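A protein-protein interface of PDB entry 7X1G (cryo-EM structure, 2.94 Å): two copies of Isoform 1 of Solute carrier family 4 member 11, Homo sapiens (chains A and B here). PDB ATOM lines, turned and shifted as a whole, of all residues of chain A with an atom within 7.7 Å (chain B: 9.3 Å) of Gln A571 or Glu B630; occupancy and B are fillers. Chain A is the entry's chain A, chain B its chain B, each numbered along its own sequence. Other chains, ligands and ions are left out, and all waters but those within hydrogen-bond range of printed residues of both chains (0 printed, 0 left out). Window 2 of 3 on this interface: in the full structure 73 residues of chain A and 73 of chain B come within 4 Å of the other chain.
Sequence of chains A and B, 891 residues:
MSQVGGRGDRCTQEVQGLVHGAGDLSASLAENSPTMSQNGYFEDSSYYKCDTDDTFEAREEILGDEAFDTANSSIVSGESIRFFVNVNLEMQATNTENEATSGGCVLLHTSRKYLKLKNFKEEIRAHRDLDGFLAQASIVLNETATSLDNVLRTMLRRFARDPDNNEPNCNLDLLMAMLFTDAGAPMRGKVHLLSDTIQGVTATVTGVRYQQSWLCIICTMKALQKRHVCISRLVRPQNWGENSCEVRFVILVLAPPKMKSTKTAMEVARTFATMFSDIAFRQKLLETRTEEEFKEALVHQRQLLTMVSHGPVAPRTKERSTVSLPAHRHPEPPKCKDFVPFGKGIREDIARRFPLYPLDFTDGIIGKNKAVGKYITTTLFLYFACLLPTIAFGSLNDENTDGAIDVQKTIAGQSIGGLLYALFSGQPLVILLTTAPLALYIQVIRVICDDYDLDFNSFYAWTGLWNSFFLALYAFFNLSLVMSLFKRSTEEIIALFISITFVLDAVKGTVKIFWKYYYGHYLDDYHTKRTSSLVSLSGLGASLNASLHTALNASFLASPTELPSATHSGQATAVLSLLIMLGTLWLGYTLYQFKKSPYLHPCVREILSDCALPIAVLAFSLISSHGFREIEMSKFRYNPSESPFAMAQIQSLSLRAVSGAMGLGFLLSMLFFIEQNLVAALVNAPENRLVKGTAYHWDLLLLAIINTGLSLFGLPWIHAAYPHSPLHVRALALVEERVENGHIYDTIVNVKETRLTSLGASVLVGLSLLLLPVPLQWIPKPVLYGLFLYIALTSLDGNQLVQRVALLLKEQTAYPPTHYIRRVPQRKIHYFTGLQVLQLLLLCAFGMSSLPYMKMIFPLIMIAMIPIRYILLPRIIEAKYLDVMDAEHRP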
ATOM      1  N   ILE A 513     -12.923  29.262 -17.232  1.00  0.00           N
ATOM      2  CA  ILE A 513     -12.754  28.647 -15.918  1.00  0.00           C
ATOM      3  C   ILE A 513     -11.292  28.292 -15.683  1.00  0.00           C
ATOM      4  O   ILE A 513     -10.737  28.557 -14.610  1.00  0.00           O
ATOM      5  CB  ILE A 513     -13.666  27.412 -15.786  1.00  0.00           C
ATOM      6  CG1 ILE A 513     -15.108  27.852 -15.521  1.00  0.00           C
ATOM      7  CG2 ILE A 513     -13.163  26.495 -14.675  1.00  0.00           C
ATOM      8  CD1 ILE A 513     -16.113  26.719 -15.527  1.00  0.00           C
ATOM      9  N   PHE A 514     -10.643  27.689 -16.683  1.00  0.00           N
ATOM     10  CA  PHE A 514      -9.231  27.344 -16.545  1.00  0.00           C
ATOM     11  C   PHE A 514      -8.375  28.591 -16.367  1.00  0.00           C
ATOM     12  O   PHE A 514      -7.469  28.619 -15.527  1.00  0.00           O
ATOM     13  CB  PHE A 514      -8.767  26.550 -17.766  1.00  0.00           C
ATOM     14  CG  PHE A 514      -8.802  25.063 -17.570  1.00  0.00           C
ATOM     15  CD1 PHE A 514     -10.010  24.387 -17.518  1.00  0.00           C
ATOM     16  CD2 PHE A 514      -7.630  24.339 -17.441  1.00  0.00           C
ATOM     17  CE1 PHE A 514     -10.045  23.019 -17.339  1.00  0.00           C
ATOM     18  CE2 PHE A 514      -7.660  22.971 -17.262  1.00  0.00           C
ATOM     19  CZ  PHE A 514      -8.869  22.310 -17.211  1.00  0.00           C
ATOM     20  N   LYS A 516      -9.195  31.533 -15.135  1.00  0.00           N
ATOM     21  CA  LYS A 516      -9.393  32.180 -13.843  1.00  0.00           C
ATOM     22  C   LYS A 516      -8.836  31.334 -12.703  1.00  0.00           C
ATOM     23  O   LYS A 516      -8.201  31.864 -11.785  1.00  0.00           O
ATOM     24  CB  LYS A 516     -10.878  32.461 -13.620  1.00  0.00           C
ATOM     25  CG  LYS A 516     -11.188  33.125 -12.288  1.00  0.00           C
ATOM     26  CD  LYS A 516     -12.643  33.552 -12.204  1.00  0.00           C
ATOM     27  CE  LYS A 516     -12.946  34.237 -10.881  1.00  0.00           C
ATOM     28  NZ  LYS A 516     -12.718  33.337  -9.718  1.00  0.00           N
ATOM     29  N   TYR A 517      -9.058  30.021 -12.745  1.00  0.00           N
ATOM     30  CA  TYR A 517      -8.709  29.138 -11.639  1.00  0.00           C
ATOM     31  C   TYR A 517      -7.394  28.400 -11.859  1.00  0.00           C
ATOM     32  O   TYR A 517      -6.497  28.469 -11.014  1.00  0.00           O
ATOM     33  CB  TYR A 517      -9.837  28.126 -11.408  1.00  0.00           C
ATOM     34  CG  TYR A 517     -11.095  28.734 -10.832  1.00  0.00           C
ATOM     35  CD1 TYR A 517     -11.173  29.077  -9.489  1.00  0.00           C
ATOM     36  CD2 TYR A 517     -12.206  28.967 -11.631  1.00  0.00           C
ATOM     37  CE1 TYR A 517     -12.320  29.632  -8.959  1.00  0.00           C
ATOM     38  CE2 TYR A 517     -13.358  29.523 -11.111  1.00  0.00           C
ATOM     39  CZ  TYR A 517     -13.409  29.853  -9.775  1.00  0.00           C
ATOM     40  OH  TYR A 517     -14.555  30.406  -9.251  1.00  0.00           O
ATOM     41  N   TYR A 518      -7.259  27.689 -12.981  1.00  0.00           N
ATOM     42  CA  TYR A 518      -6.066  26.875 -13.196  1.00  0.00           C
ATOM     43  C   TYR A 518      -4.809  27.734 -13.234  1.00  0.00           C
ATOM     44  O   TYR A 518      -3.792  27.386 -12.623  1.00  0.00           O
ATOM     45  CB  TYR A 518      -6.204  26.078 -14.493  1.00  0.00           C
ATOM     46  CG  TYR A 518      -5.160  24.999 -14.664  1.00  0.00           C
ATOM     47  CD1 TYR A 518      -5.381  23.713 -14.193  1.00  0.00           C
ATOM     48  CD2 TYR A 518      -3.955  25.266 -15.297  1.00  0.00           C
ATOM     49  CE1 TYR A 518      -4.431  22.724 -14.348  1.00  0.00           C
ATOM     50  CE2 TYR A 518      -2.999  24.284 -15.456  1.00  0.00           C
ATOM     51  CZ  TYR A 518      -3.242  23.015 -14.979  1.00  0.00           C
ATOM     52  OH  TYR A 518      -2.294  22.032 -15.135  1.00  0.00           O
ATOM     53  N   TYR A 519      -4.856  28.859 -13.943  1.00  0.00           N
ATOM     54  CA  TYR A 519      -3.706  29.740 -14.087  1.00  0.00           C
ATOM     55  C   TYR A 519      -3.692  30.873 -13.070  1.00  0.00           C
ATOM     56  O   TYR A 519      -2.776  31.700 -13.096  1.00  0.00           O
ATOM     57  CB  TYR A 519      -3.665  30.315 -15.505  1.00  0.00           C
ATOM     58  CG  TYR A 519      -3.437  29.267 -16.570  1.00  0.00           C
ATOM     59  CD1 TYR A 519      -2.254  28.543 -16.618  1.00  0.00           C
ATOM     60  CD2 TYR A 519      -4.408  28.994 -17.523  1.00  0.00           C
ATOM     61  CE1 TYR A 519      -2.041  27.582 -17.586  1.00  0.00           C
ATOM     62  CE2 TYR A 519      -4.205  28.035 -18.497  1.00  0.00           C
ATOM     63  CZ  TYR A 519      -3.020  27.333 -18.523  1.00  0.00           C
ATOM     64  OH  TYR A 519      -2.813  26.376 -19.490  1.00  0.00           O
ATOM     65  N   GLY A 520      -4.681  30.934 -12.180  1.00  0.00           N
ATOM     66  CA  GLY A 520      -4.673  31.929 -11.125  1.00  0.00           C
ATOM     67  C   GLY A 520      -4.819  33.357 -11.593  1.00  0.00           C
ATOM     68  O   GLY A 520      -4.434  34.276 -10.866  1.00  0.00           O
ATOM     69  N   TYR A 522      -7.045  35.724 -11.607  1.00  0.00           N
ATOM     70  CA  TYR A 522      -8.285  36.247 -11.046  1.00  0.00           C
ATOM     71  C   TYR A 522      -8.574  37.640 -11.598  1.00  0.00           C
ATOM     72  O   TYR A 522      -8.988  38.535 -10.862  1.00  0.00           O
ATOM     73  CB  TYR A 522      -8.210  36.294  -9.517  1.00  0.00           C
ATOM     74  CG  TYR A 522      -8.101  34.938  -8.849  1.00  0.00           C
ATOM     75  CD1 TYR A 522      -8.576  33.789  -9.468  1.00  0.00           C
ATOM     76  CD2 TYR A 522      -7.521  34.810  -7.593  1.00  0.00           C
ATOM     77  CE1 TYR A 522      -8.477  32.554  -8.856  1.00  0.00           C
ATOM     78  CE2 TYR A 522      -7.417  33.580  -6.975  1.00  0.00           C
ATOM     79  CZ  TYR A 522      -7.897  32.455  -7.611  1.00  0.00           C
ATOM     80  OH  TYR A 522      -7.796  31.227  -6.998  1.00  0.00           O
ATOM     81  N   SER A 569      -5.900  26.584  -4.845  1.00  0.00           N
ATOM     82  CA  SER A 569      -6.701  25.402  -5.137  1.00  0.00           C
ATOM     83  C   SER A 569      -7.463  25.562  -6.450  1.00  0.00           C
ATOM     84  O   SER A 569      -8.365  24.782  -6.749  1.00  0.00           O
ATOM     85  CB  SER A 569      -7.680  25.127  -3.993  1.00  0.00           C
ATOM     86  OG  SER A 569      -8.452  23.967  -4.247  1.00  0.00           O
ATOM     87  N   GLY A 570      -7.092  26.576  -7.234  1.00  0.00           N
ATOM     88  CA  GLY A 570      -7.774  26.814  -8.494  1.00  0.00           C
ATOM     89  C   GLY A 570      -7.603  25.687  -9.491  1.00  0.00           C
ATOM     90  O   GLY A 570      -8.524  25.389 -10.257  1.00  0.00           O
ATOM     91  N   GLN A 571      -6.432  25.050  -9.501  1.00  0.00           N
ATOM     92  CA  GLN A 571      -6.207  23.945 -10.427  1.00  0.00           C
ATOM     93  C   GLN A 571      -7.193  22.813 -10.173  1.00  0.00           C
ATOM     94  O   GLN A 571      -7.729  22.219 -11.118  1.00  0.00           O
ATOM     95  CB  GLN A 571      -4.769  23.443 -10.299  1.00  0.00           C
ATOM     96  CG  GLN A 571      -3.720  24.516 -10.529  1.00  0.00           C
ATOM     97  CD  GLN A 571      -2.318  23.949 -10.623  1.00  0.00           C
ATOM     98  OE1 GLN A 571      -2.024  22.896 -10.060  1.00  0.00           O
ATOM     99  NE2 GLN A 571      -1.445  24.647 -11.339  1.00  0.00           N
ATOM    100  N   ALA A 572      -7.443  22.501  -8.901  1.00  0.00           N
ATOM    101  CA  ALA A 572      -8.416  21.466  -8.576  1.00  0.00           C
ATOM    102  C   ALA A 572      -9.800  21.838  -9.086  1.00  0.00           C
ATOM    103  O   ALA A 572     -10.506  20.997  -9.653  1.00  0.00           O
ATOM    104  CB  ALA A 572      -8.447  21.231  -7.065  1.00  0.00           C
ATOM    105  N   THR A 573     -10.203  23.098  -8.903  1.00  0.00           N
ATOM    106  CA  THR A 573     -11.517  23.522  -9.377  1.00  0.00           C
ATOM    107  C   THR A 573     -11.615  23.410 -10.892  1.00  0.00           C
ATOM    108  O   THR A 573     -12.635  22.959 -11.419  1.00  0.00           O
ATOM    109  CB  THR A 573     -11.814  24.956  -8.937  1.00  0.00           C
ATOM    110  OG1 THR A 573     -10.970  25.866  -9.653  1.00  0.00           O
ATOM    111  CG2 THR A 573     -11.597  25.127  -7.440  1.00  0.00           C
ATOM    112  N   ALA A 574     -10.568  23.815 -11.611  1.00  0.00           N
ATOM    113  CA  ALA A 574     -10.604  23.746 -13.070  1.00  0.00           C
ATOM    114  C   ALA A 574     -10.682  22.302 -13.554  1.00  0.00           C
ATOM    115  O   ALA A 574     -11.472  21.975 -14.452  1.00  0.00           O
ATOM    116  CB  ALA A 574      -9.377  24.444 -13.655  1.00  0.00           C
ATOM    117  N   VAL A 575      -9.864  21.421 -12.973  1.00  0.00           N
ATOM    118  CA  VAL A 575      -9.873  20.024 -13.397  1.00  0.00           C
ATOM    119  C   VAL A 575     -11.217  19.384 -13.074  1.00  0.00           C
ATOM    120  O   VAL A 575     -11.765  18.616 -13.874  1.00  0.00           O
ATOM    121  CB  VAL A 575      -8.705  19.257 -12.750  1.00  0.00           C
ATOM    122  CG1 VAL A 575      -8.744  17.792 -13.152  1.00  0.00           C
ATOM    123  CG2 VAL A 575      -7.374  19.873 -13.154  1.00  0.00           C
ATOM    124  N   LEU A 576     -11.771  19.690 -11.898  1.00  0.00           N
ATOM    125  CA  LEU A 576     -13.084  19.162 -11.544  1.00  0.00           C
ATOM    126  C   LEU A 576     -14.161  19.701 -12.472  1.00  0.00           C
ATOM    127  O   LEU A 576     -15.105  18.984 -12.811  1.00  0.00           O
ATOM    128  CB  LEU A 576     -13.411  19.501 -10.091  1.00  0.00           C
ATOM    129  CG  LEU A 576     -14.714  18.910  -9.545  1.00  0.00           C
ATOM    130  CD1 LEU A 576     -14.787  17.411  -9.789  1.00  0.00           C
ATOM    131  CD2 LEU A 576     -14.856  19.218  -8.065  1.00  0.00           C
ATOM    132  N   SER A 577     -14.051  20.965 -12.880  1.00  0.00           N
ATOM    133  CA  SER A 577     -15.005  21.525 -13.829  1.00  0.00           C
ATOM    134  C   SER A 577     -14.968  20.766 -15.146  1.00  0.00           C
ATOM    135  O   SER A 577     -16.013  20.394 -15.697  1.00  0.00           O
ATOM    136  CB  SER A 577     -14.696  23.006 -14.053  1.00  0.00           C
ATOM    137  OG  SER A 577     -14.697  23.718 -12.829  1.00  0.00           O
ATOM    138  N   ILE A 631     -14.252  21.162  -2.861  1.00  0.00           N
ATOM    139  CA  ILE A 631     -13.749  21.947  -3.983  1.00  0.00           C
ATOM    140  C   ILE A 631     -14.847  22.879  -4.473  1.00  0.00           C
ATOM    141  O   ILE A 631     -15.675  22.497  -5.309  1.00  0.00           O
ATOM    142  CB  ILE A 631     -13.251  21.036  -5.120  1.00  0.00           C
ATOM    143  CG1 ILE A 631     -12.271  19.994  -4.574  1.00  0.00           C
ATOM    144  CG2 ILE A 631     -12.601  21.867  -6.220  1.00  0.00           C
ATOM    145  CD1 ILE A 631     -11.638  19.118  -5.635  1.00  0.00           C
ATOM    146  N   SER B 569      -1.958  20.764  -2.964  1.00  0.00           N
ATOM    147  CA  SER B 569      -2.423  20.555  -4.330  1.00  0.00           C
ATOM    148  C   SER B 569      -2.834  19.103  -4.555  1.00  0.00           C
ATOM    149  O   SER B 569      -3.027  18.676  -5.692  1.00  0.00           O
ATOM    150  CB  SER B 569      -1.334  20.952  -5.331  1.00  0.00           C
ATOM    151  OG  SER B 569      -1.777  20.779  -6.665  1.00  0.00           O
ATOM    152  N   GLY B 570      -2.973  18.347  -3.464  1.00  0.00           N
ATOM    153  CA  GLY B 570      -3.344  16.948  -3.587  1.00  0.00           C
ATOM    154  C   GLY B 570      -4.725  16.744  -4.176  1.00  0.00           C
ATOM    155  O   GLY B 570      -4.952  15.780  -4.912  1.00  0.00           O
ATOM    156  N   GLN B 571      -5.665  17.637  -3.861  1.00  0.00           N
ATOM    157  CA  GLN B 571      -7.011  17.508  -4.407  1.00  0.00           C
ATOM    158  C   GLN B 571      -6.991  17.575  -5.927  1.00  0.00           C
ATOM    159  O   GLN B 571      -7.691  16.809  -6.603  1.00  0.00           O
ATOM    160  CB  GLN B 571      -7.912  18.599  -3.833  1.00  0.00           C
ATOM    161  CG  GLN B 571      -7.981  18.607  -2.316  1.00  0.00           C
ATOM    162  CD  GLN B 571      -9.049  19.540  -1.785  1.00  0.00           C
ATOM    163  OE1 GLN B 571      -9.408  20.523  -2.434  1.00  0.00           O
ATOM    164  NE2 GLN B 571      -9.564  19.237  -0.600  1.00  0.00           N
ATOM    165  N   ALA B 572      -6.194  18.489  -6.483  1.00  0.00           N
ATOM    166  CA  ALA B 572      -6.079  18.580  -7.934  1.00  0.00           C
ATOM    167  C   ALA B 572      -5.532  17.286  -8.518  1.00  0.00           C
ATOM    168  O   ALA B 572      -6.034  16.797  -9.536  1.00  0.00           O
ATOM    169  CB  ALA B 572      -5.188  19.760  -8.316  1.00  0.00           C
ATOM    170  N   THR B 573      -4.506  16.711  -7.885  1.00  0.00           N
ATOM    171  CA  THR B 573      -3.939  15.464  -8.391  1.00  0.00           C
ATOM    172  C   THR B 573      -4.965  14.340  -8.348  1.00  0.00           C
ATOM    173  O   THR B 573      -5.069  13.555  -9.294  1.00  0.00           O
ATOM    174  CB  THR B 573      -2.696  15.072  -7.590  1.00  0.00           C
ATOM    175  OG1 THR B 573      -3.079  14.672  -6.269  1.00  0.00           O
ATOM    176  CG2 THR B 573      -1.708  16.227  -7.509  1.00  0.00           C
ATOM    177  N   ALA B 574      -5.733  14.244  -7.261  1.00  0.00           N
ATOM    178  CA  ALA B 574      -6.726  13.179  -7.153  1.00  0.00           C
ATOM    179  C   ALA B 574      -7.820  13.333  -8.204  1.00  0.00           C
ATOM    180  O   ALA B 574      -8.214  12.357  -8.859  1.00  0.00           O
ATOM    181  CB  ALA B 574      -7.327  13.169  -5.749  1.00  0.00           C
ATOM    182  N   VAL B 575      -8.328  14.556  -8.379  1.00  0.00           N
ATOM    183  CA  VAL B 575      -9.388  14.776  -9.358  1.00  0.00           C
ATOM    184  C   VAL B 575      -8.872  14.505 -10.764  1.00  0.00           C
ATOM    185  O   VAL B 575      -9.567  13.905 -11.594  1.00  0.00           O
ATOM    186  CB  VAL B 575      -9.960  16.200  -9.223  1.00  0.00           C
ATOM    187  CG1 VAL B 575     -11.029  16.444 -10.274  1.00  0.00           C
ATOM    188  CG2 VAL B 575     -10.537  16.413  -7.832  1.00  0.00           C
ATOM    189  N   LEU B 576      -7.643  14.940 -11.058  1.00  0.00           N
ATOM    190  CA  LEU B 576      -7.059  14.669 -12.365  1.00  0.00           C
ATOM    191  C   LEU B 576      -6.846  13.176 -12.572  1.00  0.00           C
ATOM    192  O   LEU B 576      -7.010  12.673 -13.686  1.00  0.00           O
ATOM    193  CB  LEU B 576      -5.739  15.422 -12.518  1.00  0.00           C
ATOM    194  CG  LEU B 576      -5.066  15.318 -13.889  1.00  0.00           C
ATOM    195  CD1 LEU B 576      -6.032  15.672 -15.010  1.00  0.00           C
ATOM    196  CD2 LEU B 576      -3.836  16.207 -13.945  1.00  0.00           C
ATOM    197  N   LEU B 579     -10.210  11.767 -13.469  1.00  0.00           N
ATOM    198  CA  LEU B 579     -10.574  12.175 -14.821  1.00  0.00           C
ATOM    199  C   LEU B 579      -9.782  11.397 -15.862  1.00  0.00           C
ATOM    200  O   LEU B 579     -10.344  10.941 -16.863  1.00  0.00           O
ATOM    201  CB  LEU B 579     -10.352  13.680 -14.985  1.00  0.00           C
ATOM    202  CG  LEU B 579     -10.240  14.245 -16.406  1.00  0.00           C
ATOM    203  CD1 LEU B 579     -11.589  14.226 -17.099  1.00  0.00           C
ATOM    204  CD2 LEU B 579      -9.683  15.657 -16.364  1.00  0.00           C
ATOM    205  N   ILE B 623      -1.751  13.780 -22.369  1.00  0.00           N
ATOM    206  CA  ILE B 623      -2.620  14.771 -21.737  1.00  0.00           C
ATOM    207  C   ILE B 623      -2.195  15.007 -20.292  1.00  0.00           C
ATOM    208  O   ILE B 623      -2.105  16.152 -19.832  1.00  0.00           O
ATOM    209  CB  ILE B 623      -4.090  14.324 -21.825  1.00  0.00           C
ATOM    210  CG1 ILE B 623      -4.619  14.522 -23.247  1.00  0.00           C
ATOM    211  CG2 ILE B 623      -4.944  15.097 -20.828  1.00  0.00           C
ATOM    212  CD1 ILE B 623      -5.901  13.770 -23.535  1.00  0.00           C
ATOM    213  N   SER B 624      -1.928  13.929 -19.554  1.00  0.00           N
ATOM    214  CA  SER B 624      -1.632  14.025 -18.130  1.00  0.00           C
ATOM    215  C   SER B 624      -0.182  14.385 -17.836  1.00  0.00           C
ATOM    216  O   SER B 624       0.119  14.772 -16.701  1.00  0.00           O
ATOM    217  CB  SER B 624      -1.972  12.702 -17.443  1.00  0.00           C
ATOM    218  OG  SER B 624      -1.309  12.594 -16.197  1.00  0.00           O
ATOM    219  N   SER B 625       0.719  14.271 -18.813  1.00  0.00           N
ATOM    220  CA  SER B 625       2.121  14.602 -18.608  1.00  0.00           C
ATOM    221  C   SER B 625       2.554  15.876 -19.316  1.00  0.00           C
ATOM    222  O   SER B 625       3.565  16.465 -18.922  1.00  0.00           O
ATOM    223  CB  SER B 625       3.015  13.446 -19.084  1.00  0.00           C
ATOM    224  OG  SER B 625       2.752  12.266 -18.346  1.00  0.00           O
ATOM    225  N   HIS B 626       1.824  16.312 -20.340  1.00  0.00           N
ATOM    226  CA  HIS B 626       2.136  17.538 -21.063  1.00  0.00           C
ATOM    227  C   HIS B 626       1.033  18.576 -20.937  1.00  0.00           C
ATOM    228  O   HIS B 626       1.317  19.744 -20.645  1.00  0.00           O
ATOM    229  CB  HIS B 626       2.391  17.222 -22.545  1.00  0.00           C
ATOM    230  CG  HIS B 626       3.338  18.173 -23.209  1.00  0.00           C
ATOM    231  ND1 HIS B 626       2.942  19.400 -23.695  1.00  0.00           N
ATOM    232  CD2 HIS B 626       4.663  18.076 -23.466  1.00  0.00           C
ATOM    233  CE1 HIS B 626       3.982  20.018 -24.223  1.00  0.00           C
ATOM    234  NE2 HIS B 626       5.040  19.236 -24.097  1.00  0.00           N
ATOM    235  N   GLY B 627      -0.224  18.183 -21.149  1.00  0.00           N
ATOM    236  CA  GLY B 627      -1.317  19.127 -20.985  1.00  0.00           C
ATOM    237  C   GLY B 627      -1.496  19.566 -19.545  1.00  0.00           C
ATOM    238  O   GLY B 627      -1.800  20.732 -19.276  1.00  0.00           O
ATOM    239  N   PHE B 628      -1.312  18.646 -18.602  1.00  0.00           N
ATOM    240  CA  PHE B 628      -1.458  18.911 -17.177  1.00  0.00           C
ATOM    241  C   PHE B 628      -0.133  18.708 -16.453  1.00  0.00           C
ATOM    242  O   PHE B 628      -0.081  18.158 -15.352  1.00  0.00           O
ATOM    243  CB  PHE B 628      -2.540  18.021 -16.568  1.00  0.00           C
ATOM    244  CG  PHE B 628      -3.939  18.438 -16.918  1.00  0.00           C
ATOM    245  CD1 PHE B 628      -4.474  19.612 -16.417  1.00  0.00           C
ATOM    246  CD2 PHE B 628      -4.721  17.653 -17.748  1.00  0.00           C
ATOM    247  CE1 PHE B 628      -5.762  19.995 -16.736  1.00  0.00           C
ATOM    248  CE2 PHE B 628      -6.009  18.031 -18.071  1.00  0.00           C
ATOM    249  CZ  PHE B 628      -6.530  19.204 -17.564  1.00  0.00           C
ATOM    250  N   ARG B 629       0.964  19.157 -17.070  1.00  0.00           N
ATOM    251  CA  ARG B 629       2.281  18.966 -16.471  1.00  0.00           C
ATOM    252  C   ARG B 629       2.433  19.713 -15.154  1.00  0.00           C
ATOM    253  O   ARG B 629       3.271  19.326 -14.332  1.00  0.00           O
ATOM    254  CB  ARG B 629       3.369  19.410 -17.450  1.00  0.00           C
ATOM    255  CG  ARG B 629       3.378  20.900 -17.747  1.00  0.00           C
ATOM    256  CD  ARG B 629       4.404  21.243 -18.813  1.00  0.00           C
ATOM    257  NE  ARG B 629       4.486  22.680 -19.054  1.00  0.00           N
ATOM    258  CZ  ARG B 629       3.720  23.346 -19.908  1.00  0.00           C
ATOM    259  NH1 ARG B 629       2.787  22.736 -20.624  1.00  0.00           N
ATOM    260  NH2 ARG B 629       3.893  24.656 -20.049  1.00  0.00           N
ATOM    261  N   GLU B 630       1.647  20.768 -14.930  1.00  0.00           N
ATOM    262  CA  GLU B 630       1.723  21.497 -13.670  1.00  0.00           C
ATOM    263  C   GLU B 630       1.195  20.680 -12.499  1.00  0.00           C
ATOM    264  O   GLU B 630       1.489  21.012 -11.346  1.00  0.00           O
ATOM    265  CB  GLU B 630       0.947  22.810 -13.775  1.00  0.00           C
ATOM    266  CG  GLU B 630       1.443  23.737 -14.871  1.00  0.00           C
ATOM    267  CD  GLU B 630       0.441  23.898 -15.998  1.00  0.00           C
ATOM    268  OE1 GLU B 630      -0.018  22.870 -16.539  1.00  0.00           O
ATOM    269  OE2 GLU B 630       0.113  25.053 -16.342  1.00  0.00           O
ATOM    270  N   ILE B 631       0.428  19.623 -12.766  1.00  0.00           N
ATOM    271  CA  ILE B 631      -0.126  18.780 -11.712  1.00  0.00           C
ATOM    272  C   ILE B 631       0.608  17.446 -11.698  1.00  0.00           C
ATOM    273  O   ILE B 631       0.239  16.513 -12.420  1.00  0.00           O
ATOM    274  CB  ILE B 631      -1.641  18.572 -11.905  1.00  0.00           C
ATOM    275  CG1 ILE B 631      -2.341  19.921 -12.085  1.00  0.00           C
ATOM    276  CG2 ILE B 631      -2.226  17.809 -10.723  1.00  0.00           C
ATOM    277  CD1 ILE B 631      -3.850  19.832 -12.173  1.00  0.00           C
ATOM    278  N   GLU B 632       1.650  17.347 -10.879  1.00  0.00           N
ATOM    279  CA  GLU B 632       2.363  16.088 -10.730  1.00  0.00           C
ATOM    280  C   GLU B 632       1.489  15.074 -10.005  1.00  0.00           C
ATOM    281  O   GLU B 632       0.756  15.418  -9.073  1.00  0.00           O
ATOM    282  CB  GLU B 632       3.670  16.302  -9.966  1.00  0.00           C
ATOM    283  CG  GLU B 632       3.486  16.815  -8.543  1.00  0.00           C
ATOM    284  CD  GLU B 632       3.393  15.701  -7.514  1.00  0.00           C
ATOM    285  OE1 GLU B 632       3.887  14.587  -7.787  1.00  0.00           O
ATOM    286  OE2 GLU B 632       2.823  15.942  -6.429  1.00  0.00           O
ATOM    287  N   MET B 633       1.567  13.815 -10.437  1.00  0.00           N
ATOM    288  CA  MET B 633       0.757  12.761  -9.839  1.00  0.00           C
ATOM    289  C   MET B 633       1.559  11.478  -9.664  1.00  0.00           C
ATOM    290  O   MET B 633       2.771  11.456  -9.900  1.00  0.00           O
ATOM    291  CB  MET B 633      -0.486  12.500 -10.692  1.00  0.00           C
ATOM    292  CG  MET B 633      -0.191  11.961 -12.079  1.00  0.00           C
ATOM    293  SD  MET B 633      -1.692  11.776 -13.059  1.00  0.00           S
ATOM    294  CE  MET B 633      -2.061  13.490 -13.416  1.00  0.00           C
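Of the printed residues of chain B, Gln A571 touches Glu B630 (3.9 Å) and Ile B631 (3.6 Å). Of chain A, only Tyr A518 (2.8 Å), Tyr A519 (3.5 Å) and Gln A571 (3.9 Å) come within 4 Å of Glu B630. Tyr A518 touches just these residues of chain B: Phe B628, Glu B630 and Ile B631. No residue of chain B comes within 4 Å of Gly A570. Ala A572 touches just one residue of chain B: Ala B572. Ala A574 touches none of the printed residues of chain B. Printed residues of chain B within 4 Å of Leu A576: Val B575. Of the printed residues of chain B, Tyr A519 touches Glu B630 (3.5 Å). Ile B623 touches none of the printed residues of chain A. The nearest printed residue of chain B that does not touch Gln A571 is Ser B569 (4.01 Å). The nearest printed residue of chain A that does not touch Ile B631 is Ala A572 (5.5 Å).
The backbone carbonyl oxygen of Phe A514 sits at hydrogen-bond distance from the backbone NH of Tyr A519. The backbone carbonyl oxygen (O) of Ile B623 sits at hydrogen-bond distance from the backbone NH (N) of Phe B628, at 2.9 Å.
CE2 of Phe A514 touches CE1 of Phe B628, 3.6 Å away. Tyr A518 touches Ile B631. Gln A571 touches Glu B630. Gln A571 touches Ile B631. Val A575 touches Val B575. CG1 of Val A575 touches CD2 of Leu B579, 3.97 Å away. CG2 of Val A575 touches CE1 of Phe B628, 3.9 Å away. CG2 of Val A575 touches CD1 of Ile B631, at 3.7 Å. CA of Leu A576 touches CG1 of Val B575, 3.6 Å away.
Gln A571 touches Ile B631, and with the chains exchanged Ile A631 touches Gln B571. Ala A572 touches its own counterpart, Ala B572. Val B575 touches its own counterpart, Val A575. Val A575 touches Leu B576, and with the chains exchanged Leu A576 touches Val B575. Of the 16 pairs that touch across the chains among the printed residues, 8 have their exchanged pair printed and touching as well.
The side-chain hydroxyl (OH) of Tyr A518 sits at hydrogen-bond distance from the side-chain carboxylate (OE1) of Glu B630.
Of the 18 printed residues of chain A, 8 touch a printed residue of chain B. Printed residues of chain A that touch a printed residue of chain B: Phe A514, Tyr A518, Tyr A519, Gln A571, Ala A572, Val A575, Leu A576 and Ile A631. Hydrophobic or aromatic side chains of chain A that line the printed part of chain B: Phe A514, Tyr A518, Tyr A519, Ala A572, Val A575, Leu A576 and Ile A631. Along chain A the printed residues that touch a printed residue of chain B span positions 514 to 631. Among the printed residues, 16 pairs touch across the chains.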
